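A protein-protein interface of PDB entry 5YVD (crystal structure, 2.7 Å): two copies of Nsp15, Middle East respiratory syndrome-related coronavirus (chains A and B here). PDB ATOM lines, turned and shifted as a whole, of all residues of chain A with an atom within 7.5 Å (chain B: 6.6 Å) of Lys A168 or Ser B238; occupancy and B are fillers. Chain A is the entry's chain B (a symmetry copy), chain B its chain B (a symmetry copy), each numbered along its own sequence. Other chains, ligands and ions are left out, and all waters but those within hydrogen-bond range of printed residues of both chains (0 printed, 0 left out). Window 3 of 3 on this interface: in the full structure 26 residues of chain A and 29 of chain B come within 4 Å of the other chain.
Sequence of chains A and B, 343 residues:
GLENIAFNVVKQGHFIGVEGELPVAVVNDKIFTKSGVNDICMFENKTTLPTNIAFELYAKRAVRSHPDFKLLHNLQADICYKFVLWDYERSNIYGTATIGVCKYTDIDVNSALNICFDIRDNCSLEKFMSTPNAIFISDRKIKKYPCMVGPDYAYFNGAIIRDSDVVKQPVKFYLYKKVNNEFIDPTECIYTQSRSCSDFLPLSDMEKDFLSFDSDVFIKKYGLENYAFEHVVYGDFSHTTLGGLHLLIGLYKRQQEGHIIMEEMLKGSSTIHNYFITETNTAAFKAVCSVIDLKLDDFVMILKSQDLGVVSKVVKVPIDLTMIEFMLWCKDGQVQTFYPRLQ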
ATOM      1  N   SER A  65     -17.828  37.561 -18.092  1.00  0.00           N
ATOM      2  CA  SER A  65     -17.126  37.287 -19.342  1.00  0.00           C
ATOM      3  C   SER A  65     -16.776  38.562 -20.098  1.00  0.00           C
ATOM      4  O   SER A  65     -17.407  39.595 -19.895  1.00  0.00           O
ATOM      5  CB  SER A  65     -18.013  36.445 -20.250  1.00  0.00           C
ATOM      6  OG  SER A  65     -19.198  37.143 -20.596  1.00  0.00           O
ATOM      7  N   PHE A 156     -13.264  34.471 -19.463  1.00  0.00           N
ATOM      8  CA  PHE A 156     -14.021  34.542 -18.244  1.00  0.00           C
ATOM      9  C   PHE A 156     -13.263  33.942 -17.056  1.00  0.00           C
ATOM     10  O   PHE A 156     -12.961  32.754 -17.057  1.00  0.00           O
ATOM     11  CB  PHE A 156     -15.365  33.856 -18.440  1.00  0.00           C
ATOM     12  CG  PHE A 156     -16.234  33.878 -17.219  1.00  0.00           C
ATOM     13  CD1 PHE A 156     -16.451  35.075 -16.536  1.00  0.00           C
ATOM     14  CD2 PHE A 156     -16.828  32.715 -16.751  1.00  0.00           C
ATOM     15  CE1 PHE A 156     -17.232  35.115 -15.406  1.00  0.00           C
ATOM     16  CE2 PHE A 156     -17.621  32.746 -15.620  1.00  0.00           C
ATOM     17  CZ  PHE A 156     -17.825  33.948 -14.946  1.00  0.00           C
ATOM     18  N   ILE A 161     -13.801  30.579 -22.944  1.00  0.00           N
ATOM     19  CA  ILE A 161     -15.131  29.987 -22.897  1.00  0.00           C
ATOM     20  C   ILE A 161     -15.793  30.060 -24.303  1.00  0.00           C
ATOM     21  O   ILE A 161     -15.843  31.115 -24.959  1.00  0.00           O
ATOM     22  CB  ILE A 161     -15.929  30.638 -21.736  1.00  0.00           C
ATOM     23  CG1 ILE A 161     -17.261  29.967 -21.569  1.00  0.00           C
ATOM     24  CG2 ILE A 161     -16.146  32.141 -21.924  1.00  0.00           C
ATOM     25  CD1 ILE A 161     -17.125  28.578 -21.021  1.00  0.00           C
ATOM     26  N   SER A 164     -22.101  28.677 -27.238  1.00  0.00           N
ATOM     27  CA  SER A 164     -22.966  27.503 -27.370  1.00  0.00           C
ATOM     28  C   SER A 164     -24.350  27.713 -26.729  1.00  0.00           C
ATOM     29  O   SER A 164     -24.551  28.662 -25.976  1.00  0.00           O
ATOM     30  CB  SER A 164     -22.325  26.305 -26.707  1.00  0.00           C
ATOM     31  OG  SER A 164     -22.665  26.282 -25.337  1.00  0.00           O
ATOM     32  N   ASP A 165     -25.285  26.801 -27.008  1.00  0.00           N
ATOM     33  CA  ASP A 165     -26.630  26.800 -26.400  1.00  0.00           C
ATOM     34  C   ASP A 165     -26.719  26.970 -24.858  1.00  0.00           C
ATOM     35  O   ASP A 165     -27.740  27.445 -24.345  1.00  0.00           O
ATOM     36  CB  ASP A 165     -27.301  25.458 -26.715  1.00  0.00           C
ATOM     37  CG  ASP A 165     -27.916  25.412 -28.094  1.00  0.00           C
ATOM     38  OD1 ASP A 165     -28.456  26.450 -28.525  1.00  0.00           O
ATOM     39  OD2 ASP A 165     -27.879  24.330 -28.728  1.00  0.00           O
ATOM     40  N   VAL A 166     -25.667  26.554 -24.133  1.00  0.00           N
ATOM     41  CA  VAL A 166     -25.725  26.328 -22.675  1.00  0.00           C
ATOM     42  C   VAL A 166     -24.955  27.363 -21.852  1.00  0.00           C
ATOM     43  O   VAL A 166     -24.897  27.281 -20.619  1.00  0.00           O
ATOM     44  CB  VAL A 166     -25.156  24.939 -22.302  1.00  0.00           C
ATOM     45  CG1 VAL A 166     -26.002  23.833 -22.891  1.00  0.00           C
ATOM     46  CG2 VAL A 166     -23.707  24.796 -22.755  1.00  0.00           C
ATOM     47  N   VAL A 167     -24.361  28.335 -22.527  1.00  0.00           N
ATOM     48  CA  VAL A 167     -23.451  29.262 -21.865  1.00  0.00           C
ATOM     49  C   VAL A 167     -24.256  30.296 -21.059  1.00  0.00           C
ATOM     50  O   VAL A 167     -25.286  30.781 -21.514  1.00  0.00           O
ATOM     51  CB  VAL A 167     -22.496  29.883 -22.907  1.00  0.00           C
ATOM     52  CG1 VAL A 167     -23.091  31.119 -23.570  1.00  0.00           C
ATOM     53  CG2 VAL A 167     -21.159  30.179 -22.271  1.00  0.00           C
ATOM     54  N   LYS A 168     -23.822  30.585 -19.839  1.00  0.00           N
ATOM     55  CA  LYS A 168     -24.591  31.478 -18.948  1.00  0.00           C
ATOM     56  C   LYS A 168     -23.979  32.866 -18.763  1.00  0.00           C
ATOM     57  O   LYS A 168     -24.594  33.757 -18.191  1.00  0.00           O
ATOM     58  CB  LYS A 168     -24.852  30.816 -17.586  1.00  0.00           C
ATOM     59  CG  LYS A 168     -25.924  29.759 -17.645  1.00  0.00           C
ATOM     60  CD  LYS A 168     -27.103  30.241 -18.483  1.00  0.00           C
ATOM     61  CE  LYS A 168     -28.432  29.665 -18.033  1.00  0.00           C
ATOM     62  NZ  LYS A 168     -29.535  30.586 -18.386  1.00  0.00           N
ATOM     63  N   GLN A 169     -22.768  33.039 -19.261  1.00  0.00           N
ATOM     64  CA  GLN A 169     -22.221  34.346 -19.449  1.00  0.00           C
ATOM     65  C   GLN A 169     -22.326  34.602 -20.938  1.00  0.00           C
ATOM     66  O   GLN A 169     -22.351  33.645 -21.715  1.00  0.00           O
ATOM     67  CB  GLN A 169     -20.779  34.355 -18.991  1.00  0.00           C
ATOM     68  CG  GLN A 169     -20.654  34.416 -17.479  1.00  0.00           C
ATOM     69  CD  GLN A 169     -20.814  35.828 -16.929  1.00  0.00           C
ATOM     70  OE1 GLN A 169     -20.132  36.737 -17.331  1.00  0.00           O
ATOM     71  NE2 GLN A 169     -21.690  35.993 -15.991  1.00  0.00           N
ATOM     72  N   PRO A 170     -22.389  35.883 -21.348  1.00  0.00           N
ATOM     73  CA  PRO A 170     -22.333  36.212 -22.760  1.00  0.00           C
ATOM     74  C   PRO A 170     -20.973  35.844 -23.398  1.00  0.00           C
ATOM     75  O   PRO A 170     -19.920  36.099 -22.816  1.00  0.00           O
ATOM     76  CB  PRO A 170     -22.559  37.731 -22.768  1.00  0.00           C
ATOM     77  CG  PRO A 170     -22.164  38.204 -21.443  1.00  0.00           C
ATOM     78  CD  PRO A 170     -22.417  37.084 -20.498  1.00  0.00           C
ATOM     79  N   VAL A 171     -21.003  35.240 -24.586  1.00  0.00           N
ATOM     80  CA  VAL A 171     -19.763  34.929 -25.340  1.00  0.00           C
ATOM     81  C   VAL A 171     -19.659  35.717 -26.646  1.00  0.00           C
ATOM     82  O   VAL A 171     -18.593  36.220 -26.997  1.00  0.00           O
ATOM     83  CB  VAL A 171     -19.657  33.422 -25.622  1.00  0.00           C
ATOM     84  CG1 VAL A 171     -18.512  33.130 -26.584  1.00  0.00           C
ATOM     85  CG2 VAL A 171     -19.471  32.667 -24.303  1.00  0.00           C
ATOM     86  N   ASP B 236     -24.831  21.565  -9.780  1.00  0.00           N
ATOM     87  CA  ASP B 236     -25.693  22.017 -10.854  1.00  0.00           C
ATOM     88  C   ASP B 236     -24.989  23.163 -11.586  1.00  0.00           C
ATOM     89  O   ASP B 236     -24.633  24.181 -10.965  1.00  0.00           O
ATOM     90  CB  ASP B 236     -26.984  22.506 -10.225  1.00  0.00           C
ATOM     91  CG  ASP B 236     -27.976  23.035 -11.220  1.00  0.00           C
ATOM     92  OD1 ASP B 236     -27.637  23.213 -12.396  1.00  0.00           O
ATOM     93  OD2 ASP B 236     -29.121  23.295 -10.790  1.00  0.00           O
ATOM     94  N   PHE B 237     -24.819  23.000 -12.898  1.00  0.00           N
ATOM     95  CA  PHE B 237     -24.020  23.920 -13.711  1.00  0.00           C
ATOM     96  C   PHE B 237     -24.760  24.571 -14.861  1.00  0.00           C
ATOM     97  O   PHE B 237     -24.137  25.142 -15.741  1.00  0.00           O
ATOM     98  CB  PHE B 237     -22.786  23.191 -14.258  1.00  0.00           C
ATOM     99  CG  PHE B 237     -22.007  22.514 -13.194  1.00  0.00           C
ATOM    100  CD1 PHE B 237     -21.120  23.258 -12.383  1.00  0.00           C
ATOM    101  CD2 PHE B 237     -22.194  21.168 -12.944  1.00  0.00           C
ATOM    102  CE1 PHE B 237     -20.429  22.642 -11.365  1.00  0.00           C
ATOM    103  CE2 PHE B 237     -21.496  20.559 -11.933  1.00  0.00           C
ATOM    104  CZ  PHE B 237     -20.623  21.295 -11.141  1.00  0.00           C
ATOM    105  N   SER B 238     -26.077  24.540 -14.835  1.00  0.00           N
ATOM    106  CA  SER B 238     -26.866  25.026 -15.968  1.00  0.00           C
ATOM    107  C   SER B 238     -27.290  26.476 -15.776  1.00  0.00           C
ATOM    108  O   SER B 238     -27.944  27.048 -16.640  1.00  0.00           O
ATOM    109  CB  SER B 238     -28.099  24.151 -16.123  1.00  0.00           C
ATOM    110  OG  SER B 238     -28.688  24.017 -14.850  1.00  0.00           O
ATOM    111  N   HIS B 239     -26.916  27.064 -14.647  1.00  0.00           N
ATOM    112  CA  HIS B 239     -27.411  28.366 -14.257  1.00  0.00           C
ATOM    113  C   HIS B 239     -26.275  29.324 -14.056  1.00  0.00           C
ATOM    114  O   HIS B 239     -25.132  28.936 -13.871  1.00  0.00           O
ATOM    115  CB  HIS B 239     -28.198  28.283 -12.952  1.00  0.00           C
ATOM    116  CG  HIS B 239     -29.495  27.571 -13.088  1.00  0.00           C
ATOM    117  ND1 HIS B 239     -29.625  26.217 -12.859  1.00  0.00           N
ATOM    118  CD2 HIS B 239     -30.719  28.012 -13.453  1.00  0.00           C
ATOM    119  CE1 HIS B 239     -30.877  25.854 -13.065  1.00  0.00           C
ATOM    120  NE2 HIS B 239     -31.564  26.925 -13.425  1.00  0.00           N
ATOM    121  N   THR B 240     -26.635  30.594 -14.052  1.00  0.00           N
ATOM    122  CA  THR B 240     -25.671  31.650 -14.027  1.00  0.00           C
ATOM    123  C   THR B 240     -24.875  31.563 -12.726  1.00  0.00           C
ATOM    124  O   THR B 240     -23.644  31.674 -12.713  1.00  0.00           O
ATOM    125  CB  THR B 240     -26.339  33.021 -14.288  1.00  0.00           C
ATOM    126  OG1 THR B 240     -25.367  34.042 -14.090  1.00  0.00           O
ATOM    127  CG2 THR B 240     -27.579  33.265 -13.364  1.00  0.00           C
ATOM    128  N   THR B 241     -25.565  31.276 -11.632  1.00  0.00           N
ATOM    129  CA  THR B 241     -24.864  30.960 -10.411  1.00  0.00           C
ATOM    130  C   THR B 241     -24.761  29.463 -10.283  1.00  0.00           C
ATOM    131  O   THR B 241     -25.723  28.745 -10.491  1.00  0.00           O
ATOM    132  CB  THR B 241     -25.537  31.566  -9.202  1.00  0.00           C
ATOM    133  OG1 THR B 241     -25.573  32.982  -9.385  1.00  0.00           O
ATOM    134  CG2 THR B 241     -24.731  31.273  -7.990  1.00  0.00           C
ATOM    135  N   LEU B 242     -23.559  29.007  -9.975  1.00  0.00           N
ATOM    136  CA  LEU B 242     -23.232  27.601  -9.916  1.00  0.00           C
ATOM    137  C   LEU B 242     -23.848  27.025  -8.641  1.00  0.00           C
ATOM    138  O   LEU B 242     -23.652  27.572  -7.566  1.00  0.00           O
ATOM    139  CB  LEU B 242     -21.717  27.458  -9.932  1.00  0.00           C
ATOM    140  CG  LEU B 242     -21.152  26.053  -9.897  1.00  0.00           C
ATOM    141  CD1 LEU B 242     -19.704  26.053 -10.395  1.00  0.00           C
ATOM    142  CD2 LEU B 242     -21.271  25.431  -8.506  1.00  0.00           C
ATOM    143  N   GLY B 243     -24.575  25.912  -8.782  1.00  0.00           N
ATOM    144  CA  GLY B 243     -25.491  25.425  -7.750  1.00  0.00           C
ATOM    145  C   GLY B 243     -24.956  24.293  -6.888  1.00  0.00           C
ATOM    146  O   GLY B 243     -24.438  23.288  -7.399  1.00  0.00           O
ATOM    147  N   ASN B 281     -17.625  25.219 -19.352  1.00  0.00           N
ATOM    148  CA  ASN B 281     -18.522  25.048 -20.505  1.00  0.00           C
ATOM    149  C   ASN B 281     -19.729  25.942 -20.395  1.00  0.00           C
ATOM    150  O   ASN B 281     -20.139  26.555 -21.380  1.00  0.00           O
ATOM    151  CB  ASN B 281     -19.020  23.618 -20.651  1.00  0.00           C
ATOM    152  CG  ASN B 281     -17.922  22.656 -20.962  1.00  0.00           C
ATOM    153  OD1 ASN B 281     -17.156  22.866 -21.897  1.00  0.00           O
ATOM    154  ND2 ASN B 281     -17.810  21.608 -20.160  1.00  0.00           N
ATOM    155  N   THR B 282     -20.314  26.001 -19.198  1.00  0.00           N
ATOM    156  CA  THR B 282     -21.546  26.749 -19.013  1.00  0.00           C
ATOM    157  C   THR B 282     -21.291  28.151 -18.526  1.00  0.00           C
ATOM    158  O   THR B 282     -22.209  28.965 -18.456  1.00  0.00           O
ATOM    159  CB  THR B 282     -22.438  26.042 -17.991  1.00  0.00           C
ATOM    160  OG1 THR B 282     -21.849  26.138 -16.684  1.00  0.00           O
ATOM    161  CG2 THR B 282     -22.628  24.576 -18.396  1.00  0.00           C
ATOM    162  N   ALA B 283     -20.048  28.414 -18.154  1.00  0.00           N
ATOM    163  CA  ALA B 283     -19.697  29.611 -17.446  1.00  0.00           C
ATOM    164  C   ALA B 283     -20.430  29.751 -16.105  1.00  0.00           C
ATOM    165  O   ALA B 283     -20.462  30.832 -15.542  1.00  0.00           O
ATOM    166  CB  ALA B 283     -19.941  30.824 -18.321  1.00  0.00           C
ATOM    167  N   ALA B 284     -20.978  28.664 -15.570  1.00  0.00           N
ATOM    168  CA  ALA B 284     -21.600  28.726 -14.249  1.00  0.00           C
ATOM    169  C   ALA B 284     -20.508  29.040 -13.249  1.00  0.00           C
ATOM    170  O   ALA B 284     -19.393  28.517 -13.347  1.00  0.00           O
ATOM    171  CB  ALA B 284     -22.297  27.415 -13.889  1.00  0.00           C
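Hydrophobic or aromatic side chains of chain B that line the printed part of chain A: Ala B283.
Along chain B the printed residues that touch a printed residue of chain A span positions 238 to 283.
The backbone NH (N) of Ser A65 sits at hydrogen-bond distance from the side-chain amide oxygen (OE1) of Gln A169.
OG of Ser A164 lies close to N of Val A166, 3.2 Å away.
OD1 of Asp B236 is in hydrogen-bond range of OG of Ser B238 (2.8 Å).
The backbone carbonyl oxygen of Phe B237 lies within hydrogen-bond range of the side-chain hydroxyl of Thr B282 (2.7 Å).
OG of Ser B238 is in hydrogen-bond range of ND1 of His B239 (3.1 Å).
N of Ala B284 is in hydrogen-bond range of OG1 of Thr B282 (2.9 Å).
O of Thr B282 is in hydrogen-bond range of N of Lys A168 (2.7 Å).
Printed residues of chain B within 4 Å of Ile A161: Asn B281 (3.6 Å).
Printed residues of chain B within 4 Å of Val A167: Asn B281 (3.9 Å) and Thr B282 (3.6 Å).
Lys A168 touches just these residues of chain B: Ser B238, His B239, Thr B240 and Thr B282.
Pro A170 touches none of the printed residues of chain B.
Val A171 touches none of the printed residues of chain B.
Ser B238 touches just one residue of chain A: Lys A168 (3.0 Å).
Of the printed residues of chain A, Asn B281 touches Ile A161 and Val A167.
Among the printed residues, merely in contact across the chains: Lys A168 with Ser B238, Phe A156 with Ala B283, Val A167 with Thr B282, Lys A168 with His B239, Ile A161 with Asn B281, Gln A169 with Ala B283, Lys A168 with Thr B240, Val A166 with Thr B282 and Val A167 with Asn B281.
No position is printed for both chains.
Of the 10 pairs that touch across the chains among the printed residues, none has its exchanged pair printed and touching as well.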
